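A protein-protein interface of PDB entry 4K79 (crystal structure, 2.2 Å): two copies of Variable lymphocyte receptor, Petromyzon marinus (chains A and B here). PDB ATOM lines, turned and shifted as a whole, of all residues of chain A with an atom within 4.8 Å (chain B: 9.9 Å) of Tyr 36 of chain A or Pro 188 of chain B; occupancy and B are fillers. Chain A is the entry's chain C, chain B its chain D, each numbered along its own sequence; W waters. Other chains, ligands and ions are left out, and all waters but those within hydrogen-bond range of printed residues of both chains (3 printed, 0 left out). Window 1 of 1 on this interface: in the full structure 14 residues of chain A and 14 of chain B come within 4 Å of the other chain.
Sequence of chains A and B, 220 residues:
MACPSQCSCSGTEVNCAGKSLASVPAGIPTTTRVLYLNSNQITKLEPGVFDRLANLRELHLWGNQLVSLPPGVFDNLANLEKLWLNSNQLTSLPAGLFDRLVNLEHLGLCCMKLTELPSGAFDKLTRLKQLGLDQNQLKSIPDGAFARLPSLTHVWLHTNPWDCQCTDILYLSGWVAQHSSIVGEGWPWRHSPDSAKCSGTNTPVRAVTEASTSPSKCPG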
ATOM      1  N   GLU A  13      -5.499   5.016  -1.694  1.00  0.00           N
ATOM      2  CA  GLU A  13      -4.555   4.165  -1.000  1.00  0.00           C
ATOM      3  C   GLU A  13      -3.767   4.960   0.012  1.00  0.00           C
ATOM      4  O   GLU A  13      -3.251   6.014  -0.313  1.00  0.00           O
ATOM      5  CB  GLU A  13      -3.575   3.463  -2.020  1.00  0.00           C
ATOM      6  CG  GLU A  13      -2.413   2.730  -1.403  1.00  0.00           C
ATOM      7  CD  GLU A  13      -1.618   1.957  -2.445  1.00  0.00           C
ATOM      8  OE1 GLU A  13      -2.184   1.140  -3.169  1.00  0.00           O
ATOM      9  OE2 GLU A  13      -0.390   2.153  -2.567  1.00  0.00           O
ATOM     10  N   VAL A  14      -3.646   4.384   1.222  1.00  0.00           N
ATOM     11  CA  VAL A  14      -2.938   4.981   2.326  1.00  0.00           C
ATOM     12  C   VAL A  14      -1.920   4.011   2.819  1.00  0.00           C
ATOM     13  O   VAL A  14      -2.259   2.892   3.277  1.00  0.00           O
ATOM     14  CB  VAL A  14      -3.905   5.368   3.518  1.00  0.00           C
ATOM     15  CG1 VAL A  14      -3.130   5.915   4.723  1.00  0.00           C
ATOM     16  CG2 VAL A  14      -4.974   6.362   3.040  1.00  0.00           C
ATOM     17  N   ASN A  15      -0.665   4.453   2.730  1.00  0.00           N
ATOM     18  CA  ASN A  15       0.479   3.704   3.136  1.00  0.00           C
ATOM     19  C   ASN A  15       1.118   4.180   4.417  1.00  0.00           C
ATOM     20  O   ASN A  15       1.870   5.134   4.417  1.00  0.00           O
ATOM     21  CB  ASN A  15       1.516   3.741   2.027  1.00  0.00           C
ATOM     22  CG  ASN A  15       2.711   2.917   2.342  1.00  0.00           C
ATOM     23  OD1 ASN A  15       2.795   2.297   3.396  1.00  0.00           O
ATOM     24  ND2 ASN A  15       3.658   2.894   1.420  1.00  0.00           N
ATOM     25  N   CYS A  16       0.879   3.449   5.500  1.00  0.00           N
ATOM     26  CA  CYS A  16       1.478   3.764   6.791  1.00  0.00           C
ATOM     27  C   CYS A  16       2.430   2.686   7.233  1.00  0.00           C
ATOM     28  O   CYS A  16       2.733   2.595   8.435  1.00  0.00           O
ATOM     29  CB  CYS A  16       0.350   3.892   7.843  1.00  0.00           C
ATOM     30  SG  CYS A  16      -0.793   5.237   7.552  1.00  0.00           S
ATOM     31  N   ALA A  17       2.858   1.831   6.291  1.00  0.00           N
ATOM     32  CA  ALA A  17       3.636   0.627   6.568  1.00  0.00           C
ATOM     33  C   ALA A  17       5.059   0.922   6.969  1.00  0.00           C
ATOM     34  O   ALA A  17       5.702   1.813   6.422  1.00  0.00           O
ATOM     35  CB  ALA A  17       3.641  -0.292   5.375  1.00  0.00           C
ATOM     36  N   VAL A  34      -7.646   1.093   0.237  1.00  0.00           N
ATOM     37  CA  VAL A  34      -6.544   0.180   0.560  1.00  0.00           C
ATOM     38  C   VAL A  34      -5.721   0.877   1.646  1.00  0.00           C
ATOM     39  O   VAL A  34      -5.217   1.962   1.433  1.00  0.00           O
ATOM     40  CB  VAL A  34      -5.695  -0.089  -0.682  1.00  0.00           C
ATOM     41  CG1 VAL A  34      -4.384  -0.888  -0.329  1.00  0.00           C
ATOM     42  CG2 VAL A  34      -6.532  -0.818  -1.708  1.00  0.00           C
ATOM     43  N   LEU A  35      -5.581   0.212   2.781  1.00  0.00           N
ATOM     44  CA  LEU A  35      -4.958   0.735   3.931  1.00  0.00           C
ATOM     45  C   LEU A  35      -3.853  -0.183   4.405  1.00  0.00           C
ATOM     46  O   LEU A  35      -4.102  -1.277   4.937  1.00  0.00           O
ATOM     47  CB  LEU A  35      -5.979   0.971   5.021  1.00  0.00           C
ATOM     48  CG  LEU A  35      -5.537   1.567   6.373  1.00  0.00           C
ATOM     49  CD1 LEU A  35      -4.797   2.882   6.201  1.00  0.00           C
ATOM     50  CD2 LEU A  35      -6.700   1.799   7.328  1.00  0.00           C
ATOM     51  N   TYR A  36      -2.621   0.311   4.282  1.00  0.00           N
ATOM     52  CA  TYR A  36      -1.479  -0.420   4.781  1.00  0.00           C
ATOM     53  C   TYR A  36      -1.059   0.112   6.139  1.00  0.00           C
ATOM     54  O   TYR A  36      -0.570   1.252   6.226  1.00  0.00           O
ATOM     55  CB  TYR A  36      -0.307  -0.260   3.831  1.00  0.00           C
ATOM     56  CG  TYR A  36      -0.518  -0.872   2.476  1.00  0.00           C
ATOM     57  CD1 TYR A  36      -0.504  -2.267   2.303  1.00  0.00           C
ATOM     58  CD2 TYR A  36      -0.725  -0.061   1.367  1.00  0.00           C
ATOM     59  CE1 TYR A  36      -0.652  -2.831   1.052  1.00  0.00           C
ATOM     60  CE2 TYR A  36      -0.886  -0.594   0.103  1.00  0.00           C
ATOM     61  CZ  TYR A  36      -0.840  -1.974  -0.063  1.00  0.00           C
ATOM     62  OH  TYR A  36      -0.984  -2.492  -1.292  1.00  0.00           O
ATOM     63  N   LEU A  37      -1.282  -0.691   7.181  1.00  0.00           N
ATOM     64  CA  LEU A  37      -0.852  -0.353   8.545  1.00  0.00           C
ATOM     65  C   LEU A  37       0.096  -1.383   9.055  1.00  0.00           C
ATOM     66  O   LEU A  37       0.390  -1.429  10.265  1.00  0.00           O
ATOM     67  CB  LEU A  37      -2.046  -0.254   9.498  1.00  0.00           C
ATOM     68  CG  LEU A  37      -2.892   0.995   9.355  1.00  0.00           C
ATOM     69  CD1 LEU A  37      -4.246   0.776   9.938  1.00  0.00           C
ATOM     70  CD2 LEU A  37      -2.188   2.189  10.021  1.00  0.00           C
ATOM     71  N   ASN A  38       0.560  -2.231   8.152  1.00  0.00           N
ATOM     72  CA  ASN A  38       1.336  -3.360   8.553  1.00  0.00           C
ATOM     73  C   ASN A  38       2.771  -2.963   8.956  1.00  0.00           C
ATOM     74  O   ASN A  38       3.213  -1.864   8.646  1.00  0.00           O
ATOM     75  CB  ASN A  38       1.410  -4.332   7.394  1.00  0.00           C
ATOM     76  CG  ASN A  38       2.023  -3.697   6.152  1.00  0.00           C
ATOM     77  OD1 ASN A  38       1.332  -2.951   5.417  1.00  0.00           O
ATOM     78  ND2 ASN A  38       3.329  -3.988   5.897  1.00  0.00           N
ATOM     79  N   HIS A  60      -4.669  -4.002   5.730  1.00  0.00           N
ATOM     80  CA  HIS A  60      -3.437  -4.701   6.055  1.00  0.00           C
ATOM     81  C   HIS A  60      -2.963  -4.345   7.454  1.00  0.00           C
ATOM     82  O   HIS A  60      -2.365  -3.277   7.648  1.00  0.00           O
ATOM     83  CB  HIS A  60      -2.340  -4.315   5.076  1.00  0.00           C
ATOM     84  CG  HIS A  60      -2.567  -4.800   3.702  1.00  0.00           C
ATOM     85  ND1 HIS A  60      -3.529  -4.249   2.876  1.00  0.00           N
ATOM     86  CD2 HIS A  60      -1.933  -5.759   2.982  1.00  0.00           C
ATOM     87  CE1 HIS A  60      -3.480  -4.859   1.706  1.00  0.00           C
ATOM     88  NE2 HIS A  60      -2.527  -5.788   1.758  1.00  0.00           N
ATOM     89  N   LYS B  82      -4.482  -6.282 -13.315  1.00  0.00           N
ATOM     90  CA  LYS B  82      -3.115  -6.116 -12.848  1.00  0.00           C
ATOM     91  C   LYS B  82      -2.197  -6.874 -13.764  1.00  0.00           C
ATOM     92  O   LYS B  82      -2.365  -8.060 -13.960  1.00  0.00           O
ATOM     93  CB  LYS B  82      -2.940  -6.683 -11.423  1.00  0.00           C
ATOM     94  CG  LYS B  82      -3.830  -5.986 -10.396  1.00  0.00           C
ATOM     95  CD  LYS B  82      -3.436  -6.331  -8.977  1.00  0.00           C
ATOM     96  CE  LYS B  82      -4.537  -5.881  -8.100  1.00  0.00           C
ATOM     97  NZ  LYS B  82      -4.089  -5.864  -6.702  1.00  0.00           N
ATOM     98  N   TRP B  84       1.894  -7.427 -14.192  1.00  0.00           N
ATOM     99  CA  TRP B  84       3.227  -7.282 -13.634  1.00  0.00           C
ATOM    100  C   TRP B  84       4.283  -7.883 -14.553  1.00  0.00           C
ATOM    101  O   TRP B  84       4.460  -9.082 -14.610  1.00  0.00           O
ATOM    102  CB  TRP B  84       3.260  -7.968 -12.294  1.00  0.00           C
ATOM    103  CG  TRP B  84       2.235  -7.415 -11.334  1.00  0.00           C
ATOM    104  CD1 TRP B  84       1.185  -8.086 -10.779  1.00  0.00           C
ATOM    105  CD2 TRP B  84       2.170  -6.087 -10.827  1.00  0.00           C
ATOM    106  NE1 TRP B  84       0.464  -7.260  -9.948  1.00  0.00           N
ATOM    107  CE2 TRP B  84       1.037  -6.019  -9.968  1.00  0.00           C
ATOM    108  CE3 TRP B  84       2.942  -4.936 -11.026  1.00  0.00           C
ATOM    109  CZ2 TRP B  84       0.668  -4.851  -9.291  1.00  0.00           C
ATOM    110  CZ3 TRP B  84       2.567  -3.763 -10.374  1.00  0.00           C
ATOM    111  CH2 TRP B  84       1.434  -3.726  -9.520  1.00  0.00           C
ATOM    112  N   HIS B 106      -3.388  -1.670 -12.663  1.00  0.00           N
ATOM    113  CA  HIS B 106      -1.984  -1.634 -12.223  1.00  0.00           C
ATOM    114  C   HIS B 106      -1.085  -2.198 -13.311  1.00  0.00           C
ATOM    115  O   HIS B 106      -1.335  -3.279 -13.868  1.00  0.00           O
ATOM    116  CB  HIS B 106      -1.730  -2.406 -10.896  1.00  0.00           C
ATOM    117  CG  HIS B 106      -2.674  -2.001  -9.785  1.00  0.00           C
ATOM    118  ND1 HIS B 106      -2.272  -1.368  -8.627  1.00  0.00           N
ATOM    119  CD2 HIS B 106      -4.016  -2.130  -9.694  1.00  0.00           C
ATOM    120  CE1 HIS B 106      -3.332  -1.118  -7.871  1.00  0.00           C
ATOM    121  NE2 HIS B 106      -4.405  -1.563  -8.505  1.00  0.00           N
ATOM    122  N   GLN B 130      -2.074   2.864 -11.274  1.00  0.00           N
ATOM    123  CA  GLN B 130      -0.705   2.712 -10.815  1.00  0.00           C
ATOM    124  C   GLN B 130       0.183   2.318 -11.946  1.00  0.00           C
ATOM    125  O   GLN B 130      -0.083   1.328 -12.601  1.00  0.00           O
ATOM    126  CB  GLN B 130      -0.651   1.711  -9.663  1.00  0.00           C
ATOM    127  CG  GLN B 130      -1.513   2.219  -8.454  1.00  0.00           C
ATOM    128  CD  GLN B 130      -1.099   1.659  -7.111  1.00  0.00           C
ATOM    129  OE1 GLN B 130       0.025   1.218  -6.914  1.00  0.00           O
ATOM    130  NE2 GLN B 130      -2.004   1.717  -6.167  1.00  0.00           N
ATOM    131  N   HIS B 154      -0.748   6.948  -8.931  1.00  0.00           N
ATOM    132  CA  HIS B 154       0.552   6.513  -8.468  1.00  0.00           C
ATOM    133  C   HIS B 154       1.450   6.203  -9.638  1.00  0.00           C
ATOM    134  O   HIS B 154       1.085   5.427 -10.492  1.00  0.00           O
ATOM    135  CB  HIS B 154       0.472   5.225  -7.633  1.00  0.00           C
ATOM    136  CG  HIS B 154      -0.414   5.328  -6.441  1.00  0.00           C
ATOM    137  ND1 HIS B 154      -1.788   5.254  -6.530  1.00  0.00           N
ATOM    138  CD2 HIS B 154      -0.123   5.495  -5.125  1.00  0.00           C
ATOM    139  CE1 HIS B 154      -2.307   5.362  -5.320  1.00  0.00           C
ATOM    140  NE2 HIS B 154      -1.320   5.500  -4.448  1.00  0.00           N
ATOM    141  N   VAL B 155       2.629   6.815  -9.653  1.00  0.00           N
ATOM    142  CA  VAL B 155       3.558   6.596 -10.713  1.00  0.00           C
ATOM    143  C   VAL B 155       4.972   6.569 -10.158  1.00  0.00           C
ATOM    144  O   VAL B 155       5.280   7.297  -9.224  1.00  0.00           O
ATOM    145  CB  VAL B 155       3.415   7.667 -11.871  1.00  0.00           C
ATOM    146  CG1 VAL B 155       3.889   9.046 -11.445  1.00  0.00           C
ATOM    147  CG2 VAL B 155       4.204   7.213 -13.147  1.00  0.00           C
ATOM    148  N   TRP B 156       5.813   5.702 -10.748  1.00  0.00           N
ATOM    149  CA  TRP B 156       7.198   5.589 -10.436  1.00  0.00           C
ATOM    150  C   TRP B 156       8.029   5.910 -11.689  1.00  0.00           C
ATOM    151  O   TRP B 156       7.856   5.293 -12.752  1.00  0.00           O
ATOM    152  CB  TRP B 156       7.565   4.163 -10.029  1.00  0.00           C
ATOM    153  CG  TRP B 156       7.032   3.590  -8.774  1.00  0.00           C
ATOM    154  CD1 TRP B 156       7.788   3.226  -7.685  1.00  0.00           C
ATOM    155  CD2 TRP B 156       5.683   3.158  -8.481  1.00  0.00           C
ATOM    156  NE1 TRP B 156       6.987   2.676  -6.730  1.00  0.00           N
ATOM    157  CE2 TRP B 156       5.690   2.644  -7.180  1.00  0.00           C
ATOM    158  CE3 TRP B 156       4.468   3.239  -9.159  1.00  0.00           C
ATOM    159  CZ2 TRP B 156       4.551   2.141  -6.568  1.00  0.00           C
ATOM    160  CZ3 TRP B 156       3.330   2.772  -8.547  1.00  0.00           C
ATOM    161  CH2 TRP B 156       3.378   2.219  -7.257  1.00  0.00           C
ATOM    162  N   HIS B 158      11.648   7.065 -11.072  1.00  0.00           N
ATOM    163  CA  HIS B 158      13.020   7.174 -10.628  1.00  0.00           C
ATOM    164  C   HIS B 158      13.949   6.158 -11.262  1.00  0.00           C
ATOM    165  O   HIS B 158      13.519   5.150 -11.823  1.00  0.00           O
ATOM    166  CB  HIS B 158      13.090   7.072  -9.104  1.00  0.00           C
ATOM    167  CG  HIS B 158      12.704   5.720  -8.579  1.00  0.00           C
ATOM    168  ND1 HIS B 158      13.575   4.647  -8.584  1.00  0.00           N
ATOM    169  CD2 HIS B 158      11.552   5.276  -8.023  1.00  0.00           C
ATOM    170  CE1 HIS B 158      12.981   3.605  -8.035  1.00  0.00           C
ATOM    171  NE2 HIS B 158      11.755   3.962  -7.684  1.00  0.00           N
ATOM    172  N   GLY B 184       6.264   8.842  -6.955  1.00  0.00           N
ATOM    173  CA  GLY B 184       6.800   8.184  -5.761  1.00  0.00           C
ATOM    174  C   GLY B 184       7.757   7.035  -5.965  1.00  0.00           C
ATOM    175  O   GLY B 184       8.348   6.842  -7.053  1.00  0.00           O
ATOM    176  N   GLU B 185       7.898   6.259  -4.908  1.00  0.00           N
ATOM    177  CA  GLU B 185       8.986   5.327  -4.828  1.00  0.00           C
ATOM    178  C   GLU B 185       8.562   4.213  -3.878  1.00  0.00           C
ATOM    179  O   GLU B 185       7.727   4.443  -3.017  1.00  0.00           O
ATOM    180  CB  GLU B 185      10.211   6.114  -4.291  1.00  0.00           C
ATOM    181  CG  GLU B 185      11.422   5.347  -3.938  1.00  0.00           C
ATOM    182  CD  GLU B 185      12.603   6.238  -3.567  1.00  0.00           C
ATOM    183  OE1 GLU B 185      12.426   7.438  -3.180  1.00  0.00           O
ATOM    184  OE2 GLU B 185      13.718   5.684  -3.644  1.00  0.00           O
ATOM    185  N   GLY B 186       9.137   3.023  -4.056  1.00  0.00           N
ATOM    186  CA  GLY B 186       8.974   1.898  -3.108  1.00  0.00           C
ATOM    187  C   GLY B 186       7.736   1.040  -3.406  1.00  0.00           C
ATOM    188  O   GLY B 186       6.998   1.316  -4.331  1.00  0.00           O
ATOM    189  N   TRP B 187       7.513   0.022  -2.585  1.00  0.00           N
ATOM    190  CA  TRP B 187       6.368  -0.852  -2.731  1.00  0.00           C
ATOM    191  C   TRP B 187       5.882  -1.257  -1.322  1.00  0.00           C
ATOM    192  O   TRP B 187       6.623  -1.907  -0.593  1.00  0.00           O
ATOM    193  CB  TRP B 187       6.743  -2.098  -3.581  1.00  0.00           C
ATOM    194  CG  TRP B 187       5.551  -2.979  -3.719  1.00  0.00           C
ATOM    195  CD1 TRP B 187       5.317  -4.149  -3.062  1.00  0.00           C
ATOM    196  CD2 TRP B 187       4.366  -2.698  -4.467  1.00  0.00           C
ATOM    197  NE1 TRP B 187       4.079  -4.655  -3.404  1.00  0.00           N
ATOM    198  CE2 TRP B 187       3.464  -3.774  -4.251  1.00  0.00           C
ATOM    199  CE3 TRP B 187       3.990  -1.665  -5.330  1.00  0.00           C
ATOM    200  CZ2 TRP B 187       2.199  -3.842  -4.872  1.00  0.00           C
ATOM    201  CZ3 TRP B 187       2.730  -1.729  -5.945  1.00  0.00           C
ATOM    202  CH2 TRP B 187       1.848  -2.815  -5.707  1.00  0.00           C
ATOM    203  N   PRO B 188       4.659  -0.813  -0.897  1.00  0.00           N
ATOM    204  CA  PRO B 188       3.755   0.050  -1.676  1.00  0.00           C
ATOM    205  C   PRO B 188       4.324   1.449  -1.877  1.00  0.00           C
ATOM    206  O   PRO B 188       5.295   1.837  -1.220  1.00  0.00           O
ATOM    207  CB  PRO B 188       2.468   0.078  -0.850  1.00  0.00           C
ATOM    208  CG  PRO B 188       2.619  -1.104   0.221  1.00  0.00           C
ATOM    209  CD  PRO B 188       4.098  -1.167   0.434  1.00  0.00           C
ATOM    210  N   TRP B 189       3.749   2.185  -2.821  1.00  0.00           N
ATOM    211  CA  TRP B 189       4.191   3.535  -3.160  1.00  0.00           C
ATOM    212  C   TRP B 189       4.390   4.424  -1.950  1.00  0.00           C
ATOM    213  O   TRP B 189       3.566   4.411  -1.019  1.00  0.00           O
ATOM    214  CB  TRP B 189       3.112   4.159  -4.024  1.00  0.00           C
ATOM    215  CG  TRP B 189       3.335   5.521  -4.521  1.00  0.00           C
ATOM    216  CD1 TRP B 189       3.863   5.846  -5.720  1.00  0.00           C
ATOM    217  CD2 TRP B 189       2.900   6.775  -3.909  1.00  0.00           C
ATOM    218  NE1 TRP B 189       3.788   7.222  -5.925  1.00  0.00           N
ATOM    219  CE2 TRP B 189       3.229   7.810  -4.815  1.00  0.00           C
ATOM    220  CE3 TRP B 189       2.262   7.105  -2.713  1.00  0.00           C
ATOM    221  CZ2 TRP B 189       2.966   9.182  -4.544  1.00  0.00           C
ATOM    222  CZ3 TRP B 189       2.001   8.460  -2.426  1.00  0.00           C
ATOM    223  CH2 TRP B 189       2.343   9.483  -3.352  1.00  0.00           C
ATOM    224  N   ARG B 190       5.468   5.201  -1.962  1.00  0.00           N
ATOM    225  CA  ARG B 190       5.610   6.311  -0.992  1.00  0.00           C
ATOM    226  C   ARG B 190       5.814   7.629  -1.748  1.00  0.00           C
ATOM    227  O   ARG B 190       6.522   7.672  -2.777  1.00  0.00           O
ATOM    228  CB  ARG B 190       6.795   6.065  -0.067  1.00  0.00           C
ATOM    229  CG  ARG B 190       6.654   4.779   0.783  1.00  0.00           C
ATOM    230  CD  ARG B 190       7.765   4.685   1.820  1.00  0.00           C
ATOM    231  NE  ARG B 190       9.068   4.579   1.206  1.00  0.00           N
ATOM    232  CZ  ARG B 190       9.553   3.480   0.632  1.00  0.00           C
ATOM    233  NH1 ARG B 190       8.836   2.358   0.559  1.00  0.00           N
ATOM    234  NH2 ARG B 190      10.775   3.506   0.102  1.00  0.00           N
ATOM    235  N   HIS B 191       5.198   8.710  -1.260  1.00  0.00           N
ATOM    236  CA  HIS B 191       5.378  10.007  -1.960  1.00  0.00           C
ATOM    237  C   HIS B 191       6.879  10.389  -2.132  1.00  0.00           C
ATOM    238  O   HIS B 191       7.638  10.400  -1.179  1.00  0.00           O
ATOM    239  CB  HIS B 191       4.651  11.060  -1.182  1.00  0.00           C
ATOM    240  CG  HIS B 191       4.593  12.382  -1.858  1.00  0.00           C
ATOM    241  ND1 HIS B 191       4.379  12.521  -3.215  1.00  0.00           N
ATOM    242  CD2 HIS B 191       4.660  13.637  -1.350  1.00  0.00           C
ATOM    243  CE1 HIS B 191       4.329  13.808  -3.510  1.00  0.00           C
ATOM    244  NE2 HIS B 191       4.511  14.503  -2.402  1.00  0.00           N
ATOM    245  N   SER B 192       7.311  10.686  -3.342  1.00  0.00           N
ATOM    246  CA  SER B 192       8.720  11.016  -3.546  1.00  0.00           C
ATOM    247  C   SER B 192       8.883  11.812  -4.845  1.00  0.00           C
ATOM    248  O   SER B 192       9.510  11.358  -5.808  1.00  0.00           O
ATOM    249  CB  SER B 192       9.597   9.757  -3.552  1.00  0.00           C
ATOM    250  OG  SER B 192      10.958  10.125  -3.450  1.00  0.00           O
HETATM  251  O   HOH W   1       1.164   0.931  -4.221  1.00  0.00           O
HETATM  252  O   HOH W   2      -1.043   6.210  -1.535  1.00  0.00           O
HETATM  253  O   HOH W   3       0.742   4.081  -1.281  1.00  0.00           O
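Of the printed residues of chain B, Glu 13 of chain A touches Gln 130 (3.1 Å), His 154 (3.9 Å) and Pro 188 (3.9 Å).
No residue of chain B comes within 4 Å of Cys 16 of chain A.
Val 34 of chain A touches none of the printed residues of chain B.
Leu 35 of chain A touches none of the printed residues of chain B.
Of chain B, only Pro 188 (3.5 Å) comes within 4 Å of Tyr 36 of chain A.
Leu 37 of chain A touches none of the printed residues of chain B.
No residue of chain B comes within 4 Å of His 60 of chain A.
Of the printed residues of chain A, Gln 130 of chain B touches Glu 13 (3.1 Å).
Printed residues of chain A within 4 Å of His 154 of chain B: Glu 13 (3.9 Å).
Pro 188 of chain B touches just these residues of chain A: Glu 13, Asn 15 and Tyr 36.
Of the printed residues of chain A, Trp 189 of chain B touches Asn 15.
Of the printed residues of chain A, Arg 190 of chain B touches Asn 15.
Hydrophobic or aromatic side chains of chain B that line the printed part of chain A: His 154 and Pro 188.
Along chain B the printed residues that touch a printed residue of chain A span positions 130 to 190.
Of the 11 printed residues of chain A, 3 touch a printed residue of chain B.
Hydrophobic or aromatic side chains of chain A that line the printed part of chain B: Tyr 36.
Among the printed residues, 7 pairs touch across the chains.
Among the printed residues, no Asp or Glu carboxylate lies within 4 Å of a Lys or Arg side-chain nitrogen of the other chain.
NE2 of Gln 130 of chain B is in hydrogen-bond range of OE1 of Glu 13 of chain A (3.1 Å).
The side-chain amide nitrogen (ND2) of Asn 15 of chain A sits at hydrogen-bond distance from the backbone carbonyl oxygen (O) of Pro 188 of chain B (3.3 Å).
The side-chain amide nitrogen of Asn 15 of chain A sits at hydrogen-bond distance from the backbone carbonyl oxygen of Trp 189 of chain B, at 2.9 Å.
Water W2 lies within hydrogen-bond range of O of Glu 13 of chain A and NE2 of His 154 of chain B.
Water W1 lies within hydrogen-bond range of the side-chain carboxylate of Glu 13 of chain A (2.6 Å), the side-chain amide oxygen of Gln 130 of chain B (2.9 Å) and the backbone NH of Trp 189 of chain B (3.2 Å).
Water W3 bridges the side-chain carboxylate of Glu 13 of chain A (2.6 Å) and the backbone carbonyl oxygen of Trp 189 of chain B (2.9 Å).
The backbone NH (N) of Tyr 36 of chain A sits at hydrogen-bond distance from the backbone carbonyl oxygen (O) of Val 14 of chain A (2.8 Å).
The side-chain amide oxygen (OD1) of Asn 15 of chain A lies within hydrogen-bond range of the backbone NH (N) of Ala 17 of chain A (2.9 Å).
The backbone NH (N) of Cys 16 of chain A sits at hydrogen-bond distance from the backbone carbonyl oxygen (O) of Tyr 36 of chain A (2.7 Å).
N of Ala 17 of chain A is in hydrogen-bond range of O of Tyr 36 of chain A, at 3.5 Å.
O of Glu 185 of chain B is in hydrogen-bond range of N of Arg 190 of chain B.
No position is printed for both chains.
Among the printed residues, merely in contact across the chains: Glu 13 of chain A with His 154 of chain B (3.9 Å), Glu 13 of chain A with Pro 188 of chain B (3.9 Å), Asn 15 of chain A with Arg 190 of chain B (3.6 Å) and Tyr 36 of chain A with Pro 188 of chain B (3.5 Å).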
